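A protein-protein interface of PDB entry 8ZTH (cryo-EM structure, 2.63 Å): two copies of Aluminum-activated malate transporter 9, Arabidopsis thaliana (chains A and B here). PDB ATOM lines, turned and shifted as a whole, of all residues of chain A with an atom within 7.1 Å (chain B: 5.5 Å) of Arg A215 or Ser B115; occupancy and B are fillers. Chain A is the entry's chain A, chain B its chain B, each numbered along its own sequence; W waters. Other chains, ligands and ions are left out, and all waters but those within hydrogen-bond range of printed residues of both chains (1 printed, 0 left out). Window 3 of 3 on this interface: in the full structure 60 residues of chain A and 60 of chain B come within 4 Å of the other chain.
Hydrophobic or aromatic side chains of chain B within 4 Å of the printed part of chain A: Ile B105 and Phe B106.
Hydrophobic or aromatic side chains of chain A within 4 Å of the printed part of chain B: Tyr A208, Ile A211 and Phe A214.
Among the printed residues, 7 pairs touch across the chains.
No position is printed for both chains.
The guanidinium group (NH2) of Arg A215 lies within hydrogen-bond range of the backbone carbonyl oxygen (O) of Ser A212, at 3.0 Å.
The backbone carbonyl oxygen (O) of Ile A211 sits at hydrogen-bond distance from the guanidinium group (NH1) of Arg A215 (3.1 Å).
The side-chain hydroxyl of Ser B118 lies within hydrogen-bond range of the backbone carbonyl oxygen of Ser B115.
The side-chain hydroxyl (OG) of Ser B115 sits at hydrogen-bond distance from the guanidinium group (NE) of Arg A215, at 3.0 Å.
Of the printed residues of chain B, Tyr A208 touches Arg B116.
Printed residues of chain B within 4 Å of Ser A212: Ser B115 (3.8 Å).
Printed residues of chain B within 4 Å of Phe A214: Phe B106 (3.6 Å).
Arg A215 touches just these residues of chain B: Phe B106 and Ser B115.
Gln A218 touches none of the printed residues of chain B.
Ser B115 touches just these residues of chain A: Ser A212 (3.8 Å) and Arg A215 (3.0 Å).
The nearest residue of chain B that does not touch Arg A215 is Ile B105 (4.4 Å).
The nearest residue of chain A that does not touch Ser B115 is Ile A211 (4.2 Å).
The nearest printed residue of chain B that does not touch Ile A211 is Ser B115 (4.2 Å).
Water W1 bridges O of Arg B116 (3.1 Å) and OH of Tyr A208 (3.5 Å).
Among the printed residues, merely in contact across the chains: Arg A215 with Phe B106 (3.3 Å), Phe A214 with Phe B106 (3.6 Å), Ser A212 with Ser B115 (3.8 Å), Ile A211 with Phe B106 (3.9 Å), Ile A211 with Ile B105 (3.9 Å) and Tyr A208 with Arg B116 (3.99 Å).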
ATOM      1  N   TYR A 208     -15.315  15.415 -27.212  1.00  0.00           N
ATOM      2  CA  TYR A 208     -14.337  14.786 -26.334  1.00  0.00           C
ATOM      3  C   TYR A 208     -14.880  13.495 -25.736  1.00  0.00           C
ATOM      4  O   TYR A 208     -14.174  12.480 -25.700  1.00  0.00           O
ATOM      5  CB  TYR A 208     -13.916  15.751 -25.227  1.00  0.00           C
ATOM      6  CG  TYR A 208     -12.903  15.155 -24.278  1.00  0.00           C
ATOM      7  CD1 TYR A 208     -11.572  15.031 -24.644  1.00  0.00           C
ATOM      8  CD2 TYR A 208     -13.280  14.706 -23.021  1.00  0.00           C
ATOM      9  CE1 TYR A 208     -10.644  14.484 -23.785  1.00  0.00           C
ATOM     10  CE2 TYR A 208     -12.358  14.156 -22.155  1.00  0.00           C
ATOM     11  CZ  TYR A 208     -11.041  14.049 -22.543  1.00  0.00           C
ATOM     12  OH  TYR A 208     -10.118  13.503 -21.684  1.00  0.00           O
ATOM     13  N   LEU A 210     -16.964  11.556 -27.016  1.00  0.00           N
ATOM     14  CA  LEU A 210     -17.111  10.519 -28.028  1.00  0.00           C
ATOM     15  C   LEU A 210     -15.787  10.032 -28.595  1.00  0.00           C
ATOM     16  O   LEU A 210     -15.687   8.861 -28.973  1.00  0.00           O
ATOM     17  CB  LEU A 210     -17.994  11.009 -29.180  1.00  0.00           C
ATOM     18  CG  LEU A 210     -19.061  10.014 -29.643  1.00  0.00           C
ATOM     19  CD1 LEU A 210     -19.706   9.328 -28.454  1.00  0.00           C
ATOM     20  CD2 LEU A 210     -20.107  10.702 -30.499  1.00  0.00           C
ATOM     21  N   ILE A 211     -14.760  10.884 -28.660  1.00  0.00           N
ATOM     22  CA  ILE A 211     -13.460  10.450 -29.169  1.00  0.00           C
ATOM     23  C   ILE A 211     -12.534   9.925 -28.081  1.00  0.00           C
ATOM     24  O   ILE A 211     -11.481   9.356 -28.404  1.00  0.00           O
ATOM     25  CB  ILE A 211     -12.762  11.595 -29.929  1.00  0.00           C
ATOM     26  CG1 ILE A 211     -13.714  12.214 -30.952  1.00  0.00           C
ATOM     27  CG2 ILE A 211     -11.506  11.095 -30.616  1.00  0.00           C
ATOM     28  CD1 ILE A 211     -13.227  13.520 -31.526  1.00  0.00           C
ATOM     29  N   SER A 212     -12.890  10.080 -26.805  1.00  0.00           N
ATOM     30  CA  SER A 212     -11.992   9.667 -25.733  1.00  0.00           C
ATOM     31  C   SER A 212     -12.228   8.239 -25.259  1.00  0.00           C
ATOM     32  O   SER A 212     -11.277   7.576 -24.828  1.00  0.00           O
ATOM     33  CB  SER A 212     -12.127  10.621 -24.543  1.00  0.00           C
ATOM     34  OG  SER A 212     -11.125  10.372 -23.576  1.00  0.00           O
ATOM     35  N   GLY A 213     -13.462   7.746 -25.321  1.00  0.00           N
ATOM     36  CA  GLY A 213     -13.755   6.408 -24.845  1.00  0.00           C
ATOM     37  C   GLY A 213     -14.041   5.390 -25.930  1.00  0.00           C
ATOM     38  O   GLY A 213     -14.619   4.336 -25.655  1.00  0.00           O
ATOM     39  N   PHE A 214     -13.639   5.686 -27.167  1.00  0.00           N
ATOM     40  CA  PHE A 214     -14.009   4.819 -28.281  1.00  0.00           C
ATOM     41  C   PHE A 214     -13.286   3.478 -28.230  1.00  0.00           C
ATOM     42  O   PHE A 214     -13.900   2.432 -28.467  1.00  0.00           O
ATOM     43  CB  PHE A 214     -13.729   5.517 -29.610  1.00  0.00           C
ATOM     44  CG  PHE A 214     -14.213   4.748 -30.804  1.00  0.00           C
ATOM     45  CD1 PHE A 214     -15.535   4.351 -30.897  1.00  0.00           C
ATOM     46  CD2 PHE A 214     -13.343   4.409 -31.826  1.00  0.00           C
ATOM     47  CE1 PHE A 214     -15.983   3.637 -31.991  1.00  0.00           C
ATOM     48  CE2 PHE A 214     -13.786   3.697 -32.923  1.00  0.00           C
ATOM     49  CZ  PHE A 214     -15.107   3.311 -33.006  1.00  0.00           C
ATOM     50  N   ARG A 215     -11.991   3.480 -27.925  1.00  0.00           N
ATOM     51  CA  ARG A 215     -11.184   2.271 -28.024  1.00  0.00           C
ATOM     52  C   ARG A 215     -11.154   1.460 -26.734  1.00  0.00           C
ATOM     53  O   ARG A 215     -10.371   0.511 -26.634  1.00  0.00           O
ATOM     54  CB  ARG A 215      -9.755   2.622 -28.446  1.00  0.00           C
ATOM     55  CG  ARG A 215      -9.663   3.413 -29.743  1.00  0.00           C
ATOM     56  CD  ARG A 215      -8.801   4.657 -29.583  1.00  0.00           C
ATOM     57  NE  ARG A 215      -9.298   5.549 -28.544  1.00  0.00           N
ATOM     58  CZ  ARG A 215     -10.062   6.609 -28.771  1.00  0.00           C
ATOM     59  NH1 ARG A 215     -10.438   6.940 -29.995  1.00  0.00           N
ATOM     60  NH2 ARG A 215     -10.454   7.358 -27.745  1.00  0.00           N
ATOM     61  N   THR A 216     -11.984   1.805 -25.753  1.00  0.00           N
ATOM     62  CA  THR A 216     -12.018   1.070 -24.493  1.00  0.00           C
ATOM     63  C   THR A 216     -13.421   0.772 -23.981  1.00  0.00           C
ATOM     64  O   THR A 216     -13.591  -0.218 -23.265  1.00  0.00           O
ATOM     65  CB  THR A 216     -11.251   1.832 -23.406  1.00  0.00           C
ATOM     66  OG1 THR A 216     -11.882   3.098 -23.171  1.00  0.00           O
ATOM     67  CG2 THR A 216      -9.811   2.062 -23.833  1.00  0.00           C
ATOM     68  N   GLY A 217     -14.426   1.578 -24.313  1.00  0.00           N
ATOM     69  CA  GLY A 217     -15.761   1.404 -23.785  1.00  0.00           C
ATOM     70  C   GLY A 217     -16.015   2.125 -22.481  1.00  0.00           C
ATOM     71  O   GLY A 217     -17.134   2.052 -21.959  1.00  0.00           O
ATOM     72  N   GLN A 218     -15.014   2.822 -21.943  1.00  0.00           N
ATOM     73  CA  GLN A 218     -15.142   3.526 -20.667  1.00  0.00           C
ATOM     74  C   GLN A 218     -15.734   4.914 -20.910  1.00  0.00           C
ATOM     75  O   GLN A 218     -15.069   5.946 -20.804  1.00  0.00           O
ATOM     76  CB  GLN A 218     -13.792   3.606 -19.964  1.00  0.00           C
ATOM     77  CG  GLN A 218     -13.184   2.260 -19.595  1.00  0.00           C
ATOM     78  CD  GLN A 218     -14.195   1.131 -19.614  1.00  0.00           C
ATOM     79  OE1 GLN A 218     -15.099   1.078 -18.781  1.00  0.00           O
ATOM     80  NE2 GLN A 218     -14.047   0.221 -20.568  1.00  0.00           N
ATOM     81  N   PHE A 219     -17.023   4.920 -21.249  1.00  0.00           N
ATOM     82  CA  PHE A 219     -17.702   6.178 -21.526  1.00  0.00           C
ATOM     83  C   PHE A 219     -18.180   6.853 -20.249  1.00  0.00           C
ATOM     84  O   PHE A 219     -18.188   8.086 -20.172  1.00  0.00           O
ATOM     85  CB  PHE A 219     -18.882   5.949 -22.471  1.00  0.00           C
ATOM     86  CG  PHE A 219     -18.479   5.691 -23.894  1.00  0.00           C
ATOM     87  CD1 PHE A 219     -17.957   6.707 -24.674  1.00  0.00           C
ATOM     88  CD2 PHE A 219     -18.632   4.436 -24.455  1.00  0.00           C
ATOM     89  CE1 PHE A 219     -17.590   6.474 -25.983  1.00  0.00           C
ATOM     90  CE2 PHE A 219     -18.267   4.196 -25.764  1.00  0.00           C
ATOM     91  CZ  PHE A 219     -17.745   5.218 -26.530  1.00  0.00           C
ATOM     92  N   ILE B 105      -7.523  10.453 -35.560  1.00  0.00           N
ATOM     93  CA  ILE B 105      -7.302   9.926 -34.215  1.00  0.00           C
ATOM     94  C   ILE B 105      -7.575   8.428 -34.180  1.00  0.00           C
ATOM     95  O   ILE B 105      -6.786   7.649 -33.633  1.00  0.00           O
ATOM     96  CB  ILE B 105      -8.168  10.679 -33.189  1.00  0.00           C
ATOM     97  CG1 ILE B 105      -7.872  12.180 -33.229  1.00  0.00           C
ATOM     98  CG2 ILE B 105      -7.936  10.126 -31.793  1.00  0.00           C
ATOM     99  CD1 ILE B 105      -6.434  12.529 -32.936  1.00  0.00           C
ATOM    100  N   PHE B 106      -8.697   7.997 -34.765  1.00  0.00           N
ATOM    101  CA  PHE B 106      -9.061   6.585 -34.674  1.00  0.00           C
ATOM    102  C   PHE B 106      -8.023   5.686 -35.338  1.00  0.00           C
ATOM    103  O   PHE B 106      -7.509   4.752 -34.711  1.00  0.00           O
ATOM    104  CB  PHE B 106     -10.443   6.337 -35.284  1.00  0.00           C
ATOM    105  CG  PHE B 106     -11.578   6.891 -34.472  1.00  0.00           C
ATOM    106  CD1 PHE B 106     -11.380   7.310 -33.169  1.00  0.00           C
ATOM    107  CD2 PHE B 106     -12.853   6.967 -35.008  1.00  0.00           C
ATOM    108  CE1 PHE B 106     -12.428   7.809 -32.421  1.00  0.00           C
ATOM    109  CE2 PHE B 106     -13.903   7.465 -34.265  1.00  0.00           C
ATOM    110  CZ  PHE B 106     -13.690   7.886 -32.970  1.00  0.00           C
ATOM    111  N   ASN B 111      -1.835   4.443 -30.255  1.00  0.00           N
ATOM    112  CA  ASN B 111      -1.307   4.603 -28.911  1.00  0.00           C
ATOM    113  C   ASN B 111      -2.431   4.859 -27.906  1.00  0.00           C
ATOM    114  O   ASN B 111      -3.473   5.418 -28.254  1.00  0.00           O
ATOM    115  CB  ASN B 111      -0.308   5.757 -28.867  1.00  0.00           C
ATOM    116  CG  ASN B 111       0.984   5.432 -29.587  1.00  0.00           C
ATOM    117  OD1 ASN B 111       1.337   4.266 -29.761  1.00  0.00           O
ATOM    118  ND2 ASN B 111       1.699   6.467 -30.012  1.00  0.00           N
ATOM    119  N   PRO B 112      -2.237   4.456 -26.646  1.00  0.00           N
ATOM    120  CA  PRO B 112      -3.301   4.663 -25.650  1.00  0.00           C
ATOM    121  C   PRO B 112      -3.490   6.121 -25.268  1.00  0.00           C
ATOM    122  O   PRO B 112      -4.632   6.582 -25.153  1.00  0.00           O
ATOM    123  CB  PRO B 112      -2.830   3.816 -24.460  1.00  0.00           C
ATOM    124  CG  PRO B 112      -1.345   3.773 -24.606  1.00  0.00           C
ATOM    125  CD  PRO B 112      -1.087   3.727 -26.086  1.00  0.00           C
ATOM    126  N   ASP B 113      -2.398   6.861 -25.063  1.00  0.00           N
ATOM    127  CA  ASP B 113      -2.495   8.249 -24.628  1.00  0.00           C
ATOM    128  C   ASP B 113      -2.893   9.194 -25.752  1.00  0.00           C
ATOM    129  O   ASP B 113      -3.414  10.277 -25.472  1.00  0.00           O
ATOM    130  CB  ASP B 113      -1.168   8.709 -24.022  1.00  0.00           C
ATOM    131  CG  ASP B 113      -0.610   7.720 -23.021  1.00  0.00           C
ATOM    132  OD1 ASP B 113      -1.410   6.987 -22.402  1.00  0.00           O
ATOM    133  OD2 ASP B 113       0.626   7.676 -22.854  1.00  0.00           O
ATOM    134  N   LEU B 114      -2.643   8.816 -27.009  1.00  0.00           N
ATOM    135  CA  LEU B 114      -2.997   9.674 -28.136  1.00  0.00           C
ATOM    136  C   LEU B 114      -4.436  10.163 -28.051  1.00  0.00           C
ATOM    137  O   LEU B 114      -4.758  11.240 -28.568  1.00  0.00           O
ATOM    138  CB  LEU B 114      -2.762   8.924 -29.451  1.00  0.00           C
ATOM    139  CG  LEU B 114      -2.602   9.734 -30.744  1.00  0.00           C
ATOM    140  CD1 LEU B 114      -3.873  10.483 -31.114  1.00  0.00           C
ATOM    141  CD2 LEU B 114      -1.427  10.697 -30.627  1.00  0.00           C
ATOM    142  N   SER B 115      -5.311   9.405 -27.394  1.00  0.00           N
ATOM    143  CA  SER B 115      -6.736   9.706 -27.368  1.00  0.00           C
ATOM    144  C   SER B 115      -7.159  10.515 -26.148  1.00  0.00           C
ATOM    145  O   SER B 115      -8.337  10.871 -26.041  1.00  0.00           O
ATOM    146  CB  SER B 115      -7.544   8.407 -27.426  1.00  0.00           C
ATOM    147  OG  SER B 115      -7.017   7.527 -28.402  1.00  0.00           O
ATOM    148  N   ARG B 116      -6.241  10.813 -25.231  1.00  0.00           N
ATOM    149  CA  ARG B 116      -6.530  11.719 -24.127  1.00  0.00           C
ATOM    150  C   ARG B 116      -6.100  13.148 -24.413  1.00  0.00           C
ATOM    151  O   ARG B 116      -6.675  14.082 -23.846  1.00  0.00           O
ATOM    152  CB  ARG B 116      -5.854  11.237 -22.838  1.00  0.00           C
ATOM    153  CG  ARG B 116      -6.435   9.947 -22.276  1.00  0.00           C
ATOM    154  CD  ARG B 116      -6.064   9.762 -20.810  1.00  0.00           C
ATOM    155  NE  ARG B 116      -4.629   9.587 -20.616  1.00  0.00           N
ATOM    156  CZ  ARG B 116      -3.814  10.531 -20.163  1.00  0.00           C
ATOM    157  NH1 ARG B 116      -4.258  11.737 -19.850  1.00  0.00           N
ATOM    158  NH2 ARG B 116      -2.520  10.256 -20.021  1.00  0.00           N
ATOM    159  N   TYR B 117      -5.106  13.336 -25.282  1.00  0.00           N
ATOM    160  CA  TYR B 117      -4.660  14.657 -25.700  1.00  0.00           C
ATOM    161  C   TYR B 117      -5.449  15.179 -26.892  1.00  0.00           C
ATOM    162  O   TYR B 117      -4.976  16.080 -27.594  1.00  0.00           O
ATOM    163  CB  TYR B 117      -3.165  14.641 -26.043  1.00  0.00           C
ATOM    164  CG  TYR B 117      -2.277  13.818 -25.130  1.00  0.00           C
ATOM    165  CD1 TYR B 117      -2.653  13.522 -23.824  1.00  0.00           C
ATOM    166  CD2 TYR B 117      -1.056  13.335 -25.581  1.00  0.00           C
ATOM    167  CE1 TYR B 117      -1.838  12.771 -22.998  1.00  0.00           C
ATOM    168  CE2 TYR B 117      -0.235  12.584 -24.764  1.00  0.00           C
ATOM    169  CZ  TYR B 117      -0.631  12.305 -23.474  1.00  0.00           C
ATOM    170  OH  TYR B 117       0.185  11.557 -22.657  1.00  0.00           O
ATOM    171  N   SER B 118      -6.639  14.631 -27.139  1.00  0.00           N
ATOM    172  CA  SER B 118      -7.469  15.064 -28.254  1.00  0.00           C
ATOM    173  C   SER B 118      -8.144  16.404 -28.010  1.00  0.00           C
ATOM    174  O   SER B 118      -8.762  16.941 -28.935  1.00  0.00           O
ATOM    175  CB  SER B 118      -8.532  14.007 -28.560  1.00  0.00           C
ATOM    176  OG  SER B 118      -9.033  13.429 -27.369  1.00  0.00           O
HETATM  177  O   HOH W   1      -7.237  15.319 -21.056  1.00  0.00           O
